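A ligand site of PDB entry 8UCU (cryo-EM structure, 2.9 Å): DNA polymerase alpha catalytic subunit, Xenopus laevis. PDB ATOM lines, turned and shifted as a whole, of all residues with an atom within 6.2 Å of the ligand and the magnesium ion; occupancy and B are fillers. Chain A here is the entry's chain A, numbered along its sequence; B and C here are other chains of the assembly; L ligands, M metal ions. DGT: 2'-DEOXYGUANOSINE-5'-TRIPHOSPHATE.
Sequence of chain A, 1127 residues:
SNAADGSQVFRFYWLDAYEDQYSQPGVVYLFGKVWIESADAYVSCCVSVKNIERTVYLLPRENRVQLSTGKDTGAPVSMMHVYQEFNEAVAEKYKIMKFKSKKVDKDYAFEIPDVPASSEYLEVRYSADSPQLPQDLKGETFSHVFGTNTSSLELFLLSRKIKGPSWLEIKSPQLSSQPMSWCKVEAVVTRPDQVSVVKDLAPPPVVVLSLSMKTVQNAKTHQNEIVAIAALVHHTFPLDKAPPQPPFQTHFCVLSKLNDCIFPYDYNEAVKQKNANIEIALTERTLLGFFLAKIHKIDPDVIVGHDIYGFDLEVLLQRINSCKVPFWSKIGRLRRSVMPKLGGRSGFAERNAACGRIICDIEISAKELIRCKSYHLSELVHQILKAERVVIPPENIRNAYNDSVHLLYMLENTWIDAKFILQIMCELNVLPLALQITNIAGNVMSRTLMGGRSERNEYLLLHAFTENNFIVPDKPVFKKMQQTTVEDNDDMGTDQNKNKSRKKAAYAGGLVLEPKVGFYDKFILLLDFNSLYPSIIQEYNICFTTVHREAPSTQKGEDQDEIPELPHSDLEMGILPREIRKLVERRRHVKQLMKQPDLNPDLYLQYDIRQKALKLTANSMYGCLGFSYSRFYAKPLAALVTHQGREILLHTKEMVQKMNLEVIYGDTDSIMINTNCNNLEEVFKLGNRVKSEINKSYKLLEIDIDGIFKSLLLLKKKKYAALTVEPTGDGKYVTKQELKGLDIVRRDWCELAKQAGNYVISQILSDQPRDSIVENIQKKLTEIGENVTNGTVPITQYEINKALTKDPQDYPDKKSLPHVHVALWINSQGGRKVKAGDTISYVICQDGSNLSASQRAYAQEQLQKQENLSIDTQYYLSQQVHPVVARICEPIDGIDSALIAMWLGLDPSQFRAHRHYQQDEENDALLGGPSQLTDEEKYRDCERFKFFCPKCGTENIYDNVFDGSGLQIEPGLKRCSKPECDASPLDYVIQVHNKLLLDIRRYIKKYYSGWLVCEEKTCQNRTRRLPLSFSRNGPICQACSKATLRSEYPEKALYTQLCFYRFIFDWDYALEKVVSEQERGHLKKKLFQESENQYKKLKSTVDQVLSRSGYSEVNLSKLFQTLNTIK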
ATOM      1  N   ASP A 528      16.550   1.584  -7.402  1.00  0.00           N
ATOM      2  CA  ASP A 528      17.316   1.554  -6.166  1.00  0.00           C
ATOM      3  C   ASP A 528      18.509   2.497  -6.275  1.00  0.00           C
ATOM      4  O   ASP A 528      19.184   2.526  -7.309  1.00  0.00           O
ATOM      5  CB  ASP A 528      17.803   0.145  -5.849  1.00  0.00           C
ATOM      6  CG  ASP A 528      18.344   0.005  -4.434  1.00  0.00           C
ATOM      7  OD1 ASP A 528      17.553  -0.287  -3.523  1.00  0.00           O
ATOM      8  OD2 ASP A 528      19.565   0.198  -4.241  1.00  0.00           O
ATOM      9  N   PHE A 529      18.765   3.247  -5.215  1.00  0.00           N
ATOM     10  CA  PHE A 529      19.911   4.135  -5.185  1.00  0.00           C
ATOM     11  C   PHE A 529      21.203   3.332  -5.027  1.00  0.00           C
ATOM     12  O   PHE A 529      21.227   2.248  -4.433  1.00  0.00           O
ATOM     13  CB  PHE A 529      19.791   5.139  -4.044  1.00  0.00           C
ATOM     14  CG  PHE A 529      19.076   6.401  -4.423  1.00  0.00           C
ATOM     15  CD1 PHE A 529      19.722   7.386  -5.149  1.00  0.00           C
ATOM     16  CD2 PHE A 529      17.756   6.606  -4.065  1.00  0.00           C
ATOM     17  CE1 PHE A 529      19.073   8.543  -5.501  1.00  0.00           C
ATOM     18  CE2 PHE A 529      17.098   7.761  -4.414  1.00  0.00           C
ATOM     19  CZ  PHE A 529      17.762   8.735  -5.128  1.00  0.00           C
ATOM     20  N   ASN A 530      22.289   3.888  -5.556  1.00  0.00           N
ATOM     21  CA  ASN A 530      23.614   3.299  -5.474  1.00  0.00           C
ATOM     22  C   ASN A 530      24.358   3.908  -4.292  1.00  0.00           C
ATOM     23  O   ASN A 530      24.580   5.123  -4.272  1.00  0.00           O
ATOM     24  CB  ASN A 530      24.390   3.528  -6.768  1.00  0.00           C
ATOM     25  CG  ASN A 530      23.991   2.574  -7.872  1.00  0.00           C
ATOM     26  OD1 ASN A 530      23.562   3.000  -8.947  1.00  0.00           O
ATOM     27  ND2 ASN A 530      24.143   1.289  -7.621  1.00  0.00           N
ATOM     28  N   SER A 531      24.748   3.073  -3.339  1.00  0.00           N
ATOM     29  CA  SER A 531      25.495   3.517  -2.164  1.00  0.00           C
ATOM     30  C   SER A 531      24.864   4.781  -1.582  1.00  0.00           C
ATOM     31  O   SER A 531      25.464   5.849  -1.540  1.00  0.00           O
ATOM     32  CB  SER A 531      26.962   3.734  -2.508  1.00  0.00           C
ATOM     33  OG  SER A 531      27.099   4.665  -3.567  1.00  0.00           O
ATOM     34  N   LEU A 532      23.622   4.622  -1.118  1.00  0.00           N
ATOM     35  CA  LEU A 532      22.806   5.785  -0.782  1.00  0.00           C
ATOM     36  C   LEU A 532      23.433   6.608   0.331  1.00  0.00           C
ATOM     37  O   LEU A 532      23.488   7.838   0.258  1.00  0.00           O
ATOM     38  CB  LEU A 532      21.394   5.352  -0.389  1.00  0.00           C
ATOM     39  CG  LEU A 532      20.475   6.497   0.041  1.00  0.00           C
ATOM     40  CD1 LEU A 532      20.330   7.515  -1.081  1.00  0.00           C
ATOM     41  CD2 LEU A 532      19.114   5.979   0.461  1.00  0.00           C
ATOM     42  N   TYR A 533      23.907   5.962   1.392  1.00  0.00           N
ATOM     43  CA  TYR A 533      24.411   6.709   2.538  1.00  0.00           C
ATOM     44  C   TYR A 533      25.811   7.234   2.259  1.00  0.00           C
ATOM     45  O   TYR A 533      26.127   8.384   2.590  1.00  0.00           O
ATOM     46  CB  TYR A 533      24.401   5.831   3.800  1.00  0.00           C
ATOM     47  CG  TYR A 533      23.037   5.739   4.451  1.00  0.00           C
ATOM     48  CD1 TYR A 533      21.872   5.822   3.711  1.00  0.00           C
ATOM     49  CD2 TYR A 533      22.921   5.559   5.828  1.00  0.00           C
ATOM     50  CE1 TYR A 533      20.637   5.732   4.298  1.00  0.00           C
ATOM     51  CE2 TYR A 533      21.688   5.477   6.427  1.00  0.00           C
ATOM     52  CZ  TYR A 533      20.545   5.560   5.656  1.00  0.00           C
ATOM     53  OH  TYR A 533      19.312   5.479   6.255  1.00  0.00           O
ATOM     54  N   PRO A 534      26.694   6.423   1.666  1.00  0.00           N
ATOM     55  CA  PRO A 534      27.961   6.984   1.162  1.00  0.00           C
ATOM     56  C   PRO A 534      27.737   8.152   0.217  1.00  0.00           C
ATOM     57  O   PRO A 534      28.437   9.170   0.294  1.00  0.00           O
ATOM     58  CB  PRO A 534      28.595   5.788   0.451  1.00  0.00           C
ATOM     59  CG  PRO A 534      28.095   4.617   1.196  1.00  0.00           C
ATOM     60  CD  PRO A 534      26.707   4.951   1.622  1.00  0.00           C
ATOM     61  N   ARG A 587      34.586  -0.061  -4.932  1.00  0.00           N
ATOM     62  CA  ARG A 587      33.469  -0.972  -5.167  1.00  0.00           C
ATOM     63  C   ARG A 587      32.950  -0.856  -6.596  1.00  0.00           C
ATOM     64  O   ARG A 587      32.623  -1.869  -7.234  1.00  0.00           O
ATOM     65  CB  ARG A 587      32.339  -0.691  -4.173  1.00  0.00           C
ATOM     66  CG  ARG A 587      31.368  -1.827  -4.023  1.00  0.00           C
ATOM     67  CD  ARG A 587      30.077  -1.385  -3.379  1.00  0.00           C
ATOM     68  NE  ARG A 587      28.939  -2.150  -3.882  1.00  0.00           N
ATOM     69  CZ  ARG A 587      27.676  -1.774  -3.773  1.00  0.00           C
ATOM     70  NH1 ARG A 587      27.336  -0.647  -3.166  1.00  0.00           N
ATOM     71  NH2 ARG A 587      26.725  -2.556  -4.279  1.00  0.00           N
ATOM     72  N   LYS A 591      32.675  -3.761  -9.456  1.00  0.00           N
ATOM     73  CA  LYS A 591      31.413  -4.063 -10.134  1.00  0.00           C
ATOM     74  C   LYS A 591      31.566  -3.976 -11.647  1.00  0.00           C
ATOM     75  O   LYS A 591      31.073  -4.836 -12.381  1.00  0.00           O
ATOM     76  CB  LYS A 591      30.314  -3.135  -9.646  1.00  0.00           C
ATOM     77  CG  LYS A 591      29.628  -3.607  -8.378  1.00  0.00           C
ATOM     78  CD  LYS A 591      28.548  -2.643  -7.934  1.00  0.00           C
ATOM     79  CE  LYS A 591      27.176  -3.299  -7.962  1.00  0.00           C
ATOM     80  NZ  LYS A 591      26.090  -2.366  -7.556  1.00  0.00           N
ATOM     81  N   GLN A 611      32.770  -7.272  -3.788  1.00  0.00           N
ATOM     82  CA  GLN A 611      31.911  -6.094  -3.895  1.00  0.00           C
ATOM     83  C   GLN A 611      31.019  -5.963  -2.669  1.00  0.00           C
ATOM     84  O   GLN A 611      30.839  -4.857  -2.143  1.00  0.00           O
ATOM     85  CB  GLN A 611      31.072  -6.196  -5.176  1.00  0.00           C
ATOM     86  CG  GLN A 611      29.728  -5.478  -5.166  1.00  0.00           C
ATOM     87  CD  GLN A 611      28.563  -6.431  -5.048  1.00  0.00           C
ATOM     88  OE1 GLN A 611      28.647  -7.601  -5.428  1.00  0.00           O
ATOM     89  NE2 GLN A 611      27.442  -5.932  -4.528  1.00  0.00           N
ATOM     90  N   LYS A 615      30.936  -2.858  -0.013  1.00  0.00           N
ATOM     91  CA  LYS A 615      29.674  -2.219   0.354  1.00  0.00           C
ATOM     92  C   LYS A 615      29.499  -2.214   1.864  1.00  0.00           C
ATOM     93  O   LYS A 615      29.134  -1.192   2.457  1.00  0.00           O
ATOM     94  CB  LYS A 615      28.510  -2.941  -0.316  1.00  0.00           C
ATOM     95  CG  LYS A 615      27.147  -2.362   0.034  1.00  0.00           C
ATOM     96  CD  LYS A 615      26.065  -2.872  -0.908  1.00  0.00           C
ATOM     97  CE  LYS A 615      25.298  -4.040  -0.329  1.00  0.00           C
ATOM     98  NZ  LYS A 615      23.860  -3.746  -0.156  1.00  0.00           N
ATOM     99  N   LEU A 616      29.757  -3.345   2.505  1.00  0.00           N
ATOM    100  CA  LEU A 616      29.611  -3.423   3.951  1.00  0.00           C
ATOM    101  C   LEU A 616      30.630  -2.565   4.667  1.00  0.00           C
ATOM    102  O   LEU A 616      30.345  -2.019   5.727  1.00  0.00           O
ATOM    103  CB  LEU A 616      29.718  -4.871   4.427  1.00  0.00           C
ATOM    104  CG  LEU A 616      28.415  -5.605   4.784  1.00  0.00           C
ATOM    105  CD1 LEU A 616      28.737  -6.952   5.405  1.00  0.00           C
ATOM    106  CD2 LEU A 616      27.551  -4.787   5.735  1.00  0.00           C
ATOM    107  N   ASN A 619      29.184   0.919   4.467  1.00  0.00           N
ATOM    108  CA  ASN A 619      28.019   1.012   5.332  1.00  0.00           C
ATOM    109  C   ASN A 619      28.412   0.984   6.800  1.00  0.00           C
ATOM    110  O   ASN A 619      27.792   1.670   7.621  1.00  0.00           O
ATOM    111  CB  ASN A 619      27.039  -0.110   5.015  1.00  0.00           C
ATOM    112  CG  ASN A 619      26.298   0.122   3.704  1.00  0.00           C
ATOM    113  OD1 ASN A 619      26.192   1.253   3.243  1.00  0.00           O
ATOM    114  ND2 ASN A 619      25.785  -0.949   3.117  1.00  0.00           N
ATOM    115  N   SER A 620      29.434   0.215   7.165  1.00  0.00           N
ATOM    116  CA  SER A 620      29.936   0.210   8.527  1.00  0.00           C
ATOM    117  C   SER A 620      30.630   1.521   8.862  1.00  0.00           C
ATOM    118  O   SER A 620      30.584   1.968  10.011  1.00  0.00           O
ATOM    119  CB  SER A 620      30.878  -0.967   8.744  1.00  0.00           C
ATOM    120  OG  SER A 620      30.307  -2.172   8.272  1.00  0.00           O
ATOM    121  N   TYR A 622      29.563   4.319   7.807  1.00  0.00           N
ATOM    122  CA  TYR A 622      28.402   5.097   8.208  1.00  0.00           C
ATOM    123  C   TYR A 622      27.949   4.720   9.613  1.00  0.00           C
ATOM    124  O   TYR A 622      27.707   5.594  10.454  1.00  0.00           O
ATOM    125  CB  TYR A 622      27.250   4.891   7.232  1.00  0.00           C
ATOM    126  CG  TYR A 622      25.902   4.903   7.933  1.00  0.00           C
ATOM    127  CD1 TYR A 622      25.401   6.077   8.485  1.00  0.00           C
ATOM    128  CD2 TYR A 622      25.153   3.750   8.055  1.00  0.00           C
ATOM    129  CE1 TYR A 622      24.186   6.089   9.131  1.00  0.00           C
ATOM    130  CE2 TYR A 622      23.939   3.752   8.699  1.00  0.00           C
ATOM    131  CZ  TYR A 622      23.457   4.921   9.241  1.00  0.00           C
ATOM    132  OH  TYR A 622      22.247   4.937   9.875  1.00  0.00           O
ATOM    133  N   GLY A 623      27.807   3.424   9.883  1.00  0.00           N
ATOM    134  CA  GLY A 623      27.176   2.989  11.116  1.00  0.00           C
ATOM    135  C   GLY A 623      27.990   3.321  12.349  1.00  0.00           C
ATOM    136  O   GLY A 623      27.432   3.658  13.396  1.00  0.00           O
ATOM    137  N   CYS A 624      29.319   3.243  12.249  1.00  0.00           N
ATOM    138  CA  CYS A 624      30.167   3.496  13.405  1.00  0.00           C
ATOM    139  C   CYS A 624      30.045   4.921  13.903  1.00  0.00           C
ATOM    140  O   CYS A 624      30.450   5.210  15.029  1.00  0.00           O
ATOM    141  CB  CYS A 624      31.618   3.166  13.064  1.00  0.00           C
ATOM    142  SG  CYS A 624      31.954   1.398  12.919  1.00  0.00           S
ATOM    143  N   ASP A 667      11.906   0.849   0.430  1.00  0.00           N
ATOM    144  CA  ASP A 667      12.606   0.582   1.695  1.00  0.00           C
ATOM    145  C   ASP A 667      13.900   1.379   1.743  1.00  0.00           C
ATOM    146  O   ASP A 667      14.979   0.878   1.438  1.00  0.00           O
ATOM    147  CB  ASP A 667      12.858  -0.914   1.846  1.00  0.00           C
ATOM    148  CG  ASP A 667      13.438  -1.265   3.207  1.00  0.00           C
ATOM    149  OD1 ASP A 667      13.558  -0.356   4.051  1.00  0.00           O
ATOM    150  OD2 ASP A 667      13.770  -2.444   3.420  1.00  0.00           O
ATOM    151  N   THR A 668      13.774   2.646   2.128  1.00  0.00           N
ATOM    152  CA  THR A 668      14.886   3.494   2.550  1.00  0.00           C
ATOM    153  C   THR A 668      15.800   3.937   1.413  1.00  0.00           C
ATOM    154  O   THR A 668      16.572   4.884   1.588  1.00  0.00           O
ATOM    155  CB  THR A 668      15.725   2.759   3.606  1.00  0.00           C
ATOM    156  OG1 THR A 668      14.882   2.314   4.669  1.00  0.00           O
ATOM    157  CG2 THR A 668      16.817   3.662   4.159  1.00  0.00           C
ATOM    158  N   ASP A 669      15.729   3.287   0.266  1.00  0.00           N
ATOM    159  CA  ASP A 669      16.414   3.818  -0.911  1.00  0.00           C
ATOM    160  C   ASP A 669      15.737   3.464  -2.228  1.00  0.00           C
ATOM    161  O   ASP A 669      16.293   3.816  -3.272  1.00  0.00           O
ATOM    162  CB  ASP A 669      17.875   3.362  -0.910  1.00  0.00           C
ATOM    163  CG  ASP A 669      18.068   2.002  -1.532  1.00  0.00           C
ATOM    164  OD1 ASP A 669      17.181   1.142  -1.397  1.00  0.00           O
ATOM    165  OD2 ASP A 669      19.144   1.796  -2.143  1.00  0.00           O
ATOM    166  P    DC B  16      31.706  -4.633  15.478  1.00  0.00           P
ATOM    167  OP1  DC B  16      31.195  -5.400  14.330  1.00  0.00           O
ATOM    168  OP2  DC B  16      33.160  -4.504  15.705  1.00  0.00           O
ATOM    169  O5'  DC B  16      31.070  -3.176  15.410  1.00  0.00           O
ATOM    170  C5'  DC B  16      29.670  -3.003  15.583  1.00  0.00           C
ATOM    171  C4'  DC B  16      29.185  -1.735  14.912  1.00  0.00           C
ATOM    172  O4'  DC B  16      29.551  -1.779  13.514  1.00  0.00           O
ATOM    173  C3'  DC B  16      27.684  -1.536  14.912  1.00  0.00           C
ATOM    174  O3'  DC B  16      27.251  -0.923  16.115  1.00  0.00           O
ATOM    175  C2'  DC B  16      27.472  -0.657  13.697  1.00  0.00           C
ATOM    176  C1'  DC B  16      28.550  -1.142  12.734  1.00  0.00           C
ATOM    177  N1   DC B  16      28.042  -2.118  11.736  1.00  0.00           N
ATOM    178  C2   DC B  16      27.162  -1.687  10.738  1.00  0.00           C
ATOM    179  O2   DC B  16      26.836  -0.494  10.702  1.00  0.00           O
ATOM    180  N3   DC B  16      26.703  -2.581   9.838  1.00  0.00           N
ATOM    181  C4   DC B  16      27.087  -3.847   9.899  1.00  0.00           C
ATOM    182  N4   DC B  16      26.604  -4.698   8.986  1.00  0.00           N
ATOM    183  C5   DC B  16      27.970  -4.313  10.910  1.00  0.00           C
ATOM    184  C6   DC B  16      28.426  -3.427  11.798  1.00  0.00           C
ATOM    185  P    DG B  17      25.717  -1.055  16.572  1.00  0.00           P
ATOM    186  OP1  DG B  17      25.585  -0.444  17.916  1.00  0.00           O
ATOM    187  OP2  DG B  17      25.301  -2.456  16.346  1.00  0.00           O
ATOM    188  O5'  DG B  17      24.926  -0.129  15.528  1.00  0.00           O
ATOM    189  C5'  DG B  17      25.165   1.260  15.494  1.00  0.00           C
ATOM    190  C4'  DG B  17      24.265   1.952  14.486  1.00  0.00           C
ATOM    191  O4'  DG B  17      24.601   1.520  13.154  1.00  0.00           O
ATOM    192  C3'  DG B  17      22.788   1.671  14.642  1.00  0.00           C
ATOM    193  O3'  DG B  17      22.196   2.575  15.557  1.00  0.00           O
ATOM    194  C2'  DG B  17      22.261   1.854  13.232  1.00  0.00           C
ATOM    195  C1'  DG B  17      23.436   1.444  12.345  1.00  0.00           C
ATOM    196  N9   DG B  17      23.338   0.099  11.802  1.00  0.00           N
ATOM    197  C8   DG B  17      23.979  -1.022  12.244  1.00  0.00           C
ATOM    198  N7   DG B  17      23.708  -2.085  11.548  1.00  0.00           N
ATOM    199  C5   DG B  17      22.824  -1.642  10.577  1.00  0.00           C
ATOM    200  C6   DG B  17      22.173  -2.341   9.535  1.00  0.00           C
ATOM    201  O6   DG B  17      22.268  -3.548   9.254  1.00  0.00           O
ATOM    202  N1   DG B  17      21.354  -1.510   8.780  1.00  0.00           N
ATOM    203  C2   DG B  17      21.186  -0.171   9.001  1.00  0.00           C
ATOM    204  N2   DG B  17      20.353   0.469   8.175  1.00  0.00           N
ATOM    205  N3   DG B  17      21.788   0.499   9.978  1.00  0.00           N
ATOM    206  C4   DG B  17      22.581  -0.290  10.721  1.00  0.00           C
ATOM    207  N1  DOC C  29      18.542  -2.489   4.817  1.00  0.00           N
ATOM    208  C2  DOC C  29      19.187  -1.998   5.891  1.00  0.00           C
ATOM    209  N3  DOC C  29      20.130  -2.699   6.503  1.00  0.00           N
ATOM    210  C4  DOC C  29      20.453  -3.914   6.092  1.00  0.00           C
ATOM    211  C5  DOC C  29      19.795  -4.459   4.979  1.00  0.00           C
ATOM    212  C6  DOC C  29      18.841  -3.734   4.354  1.00  0.00           C
ATOM    213  O2  DOC C  29      18.906  -0.880   6.295  1.00  0.00           O
ATOM    214  N4  DOC C  29      21.435  -4.632   6.740  1.00  0.00           N
ATOM    215  C1' DOC C  29      17.499  -1.695   4.168  1.00  0.00           C
ATOM    216  C2' DOC C  29      18.135  -0.590   3.308  1.00  0.00           C
ATOM    217  C3' DOC C  29      18.081  -1.205   1.896  1.00  0.00           C
ATOM    218  C4' DOC C  29      16.752  -1.997   1.963  1.00  0.00           C
ATOM    219  O4' DOC C  29      16.690  -2.517   3.307  1.00  0.00           O
ATOM    220  C5' DOC C  29      16.745  -3.122   0.935  1.00  0.00           C
ATOM    221  O5' DOC C  29      16.227  -4.306   1.530  1.00  0.00           O
ATOM    222  P   DOC C  29      16.402  -5.713   0.771  1.00  0.00           P
ATOM    223  OP1 DOC C  29      15.713  -5.654  -0.534  1.00  0.00           O
ATOM    224  OP2 DOC C  29      17.943  -6.168   0.841  1.00  0.00           O
HETATM  225  PG  DGT L   1      23.844  -0.616  -3.457  1.00  0.00           P
HETATM  226  O1G DGT L   1      22.242  -0.596  -3.611  1.00  0.00           O
HETATM  227  O2G DGT L   1      24.358  -2.133  -3.375  1.00  0.00           O
HETATM  228  O3G DGT L   1      24.457   0.051  -4.629  1.00  0.00           O
HETATM  229  O3B DGT L   1      24.224   0.176  -2.117  1.00  0.00           O
HETATM  230  PB  DGT L   1      23.303   0.753  -0.932  1.00  0.00           P
HETATM  231  O1B DGT L   1      24.185   1.627   0.076  1.00  0.00           O
HETATM  232  O2B DGT L   1      22.214   1.565  -1.515  1.00  0.00           O
HETATM  233  O3A DGT L   1      22.667  -0.484  -0.124  1.00  0.00           O
HETATM  234  PA  DGT L   1      21.150  -0.920   0.157  1.00  0.00           P
HETATM  235  O1A DGT L   1      20.301  -0.701  -1.190  1.00  0.00           O
HETATM  236  O2A DGT L   1      21.111  -2.341   0.545  1.00  0.00           O
HETATM  237  O5' DGT L   1      20.593  -0.023   1.376  1.00  0.00           O
HETATM  238  C5' DGT L   1      20.574   1.405   1.346  1.00  0.00           C
HETATM  239  C4' DGT L   1      21.056   1.980   2.683  1.00  0.00           C
HETATM  240  O4' DGT L   1      20.728   1.106   3.789  1.00  0.00           O
HETATM  241  C3' DGT L   1      22.603   2.060   2.716  1.00  0.00           C
HETATM  242  O3' DGT L   1      23.066   3.235   2.053  1.00  0.00           O
HETATM  243  C2' DGT L   1      22.835   2.155   4.234  1.00  0.00           C
HETATM  244  C1' DGT L   1      21.772   1.189   4.782  1.00  0.00           C
HETATM  245  N9  DGT L   1      22.370  -0.127   5.042  1.00  0.00           N
HETATM  246  C8  DGT L   1      22.176  -1.270   4.330  1.00  0.00           C
HETATM  247  N7  DGT L   1      22.865  -2.230   4.855  1.00  0.00           N
HETATM  248  C5  DGT L   1      23.539  -1.768   5.932  1.00  0.00           C
HETATM  249  C6  DGT L   1      24.431  -2.347   6.869  1.00  0.00           C
HETATM  250  O6  DGT L   1      24.726  -3.525   6.799  1.00  0.00           O
HETATM  251  N1  DGT L   1      24.928  -1.563   7.839  1.00  0.00           N
HETATM  252  C2  DGT L   1      24.579  -0.245   7.908  1.00  0.00           C
HETATM  253  N2  DGT L   1      25.111   0.526   8.904  1.00  0.00           N
HETATM  254  N3  DGT L   1      23.764   0.303   7.043  1.00  0.00           N
HETATM  255  C4  DGT L   1      23.226  -0.420   6.060  1.00  0.00           C
HETATM  256 MG    MG M   1      20.748   0.672  -2.829  1.00  0.00          MG
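O3G of the ligand sits at hydrogen-bond distance from ND2 of Asn 530.
O3B of the ligand is in hydrogen-bond range of N of Ser 531 (3.2 Å).
An oxygen (O1B) of the ligand is in hydrogen-bond range of the backbone NH of Leu 532 (3.3 Å).
N9 of DG 17 of chain B sits close to N2 of the ligand (3.4 Å).
The guanidinium group of Arg 587 lies within salt-bridge range of an oxygen (O2G) of the ligand (2.6 Å).
The backbone NH of Tyr 533 lies within hydrogen-bond range of an oxygen (O3') of the ligand (2.9 Å).
The side-chain amino group (NZ) of Lys 615 is in salt-bridge range of an oxygen (O2A) of the ligand (3.2 Å).
The backbone carbonyl oxygen (O) of Asn 619 lies within hydrogen-bond range of a nitrogen (N2) of the ligand, 3.2 Å away.
N2 of the ligand sits at hydrogen-bond distance from O2 of DC 16 of chain B (2.7 Å).
The magnesium ion is bound by OD2 of Asp 528 (1.9 Å).
The magnesium ion is bound by OD2 of Asp 669.
O1G of the ligand binds the magnesium ion (2.1 Å).
O2B of the ligand is bound to the magnesium ion, 2.2 Å away.
The magnesium ion is bound by an oxygen (O1A) of the ligand, 2.2 Å away.
The backbone carbonyl oxygen (O) of Phe 529 is bound to the magnesium ion.
N3 of DOC 29 of chain C lies close to a nitrogen (N7) of the ligand.
Residues that only touch the ligand: Leu 616 (3.3 Å), Tyr 622 (3.3 Å) and Gly 623 (3.9 Å).
Hydrophobic or aromatic side chains that line the ligand: Leu 532, Tyr 533, Leu 616 and Tyr 622.
Within 4 Å of the ligand: Asp 528, Phe 529, Asn 530, Ser 531, Leu 532, Tyr 533, Arg 587, Lys 615, Leu 616, Asn 619, Tyr 622, Gly 623, Asp 669, DC 16 of chain B, DG 17 of chain B and DOC 29 of chain C.
Three residues have an atom within 4 Å of the magnesium ion: Asp 528, Phe 529 and Asp 669.
The side-chain amide nitrogen of Gln 611 lies close to the guanidinium group of Arg 587 (3.5 Å).
N2 of DG 17 of chain B lies close to O2 of DOC 29 of chain C (2.7 Å).
The backbone carbonyl oxygen of Leu 616 sits at hydrogen-bond distance from the side-chain hydroxyl of Ser 620.
The backbone carbonyl oxygen (O) of Lys 615 lies close to the side-chain amide nitrogen (ND2) of Asn 619 (3.4 Å).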
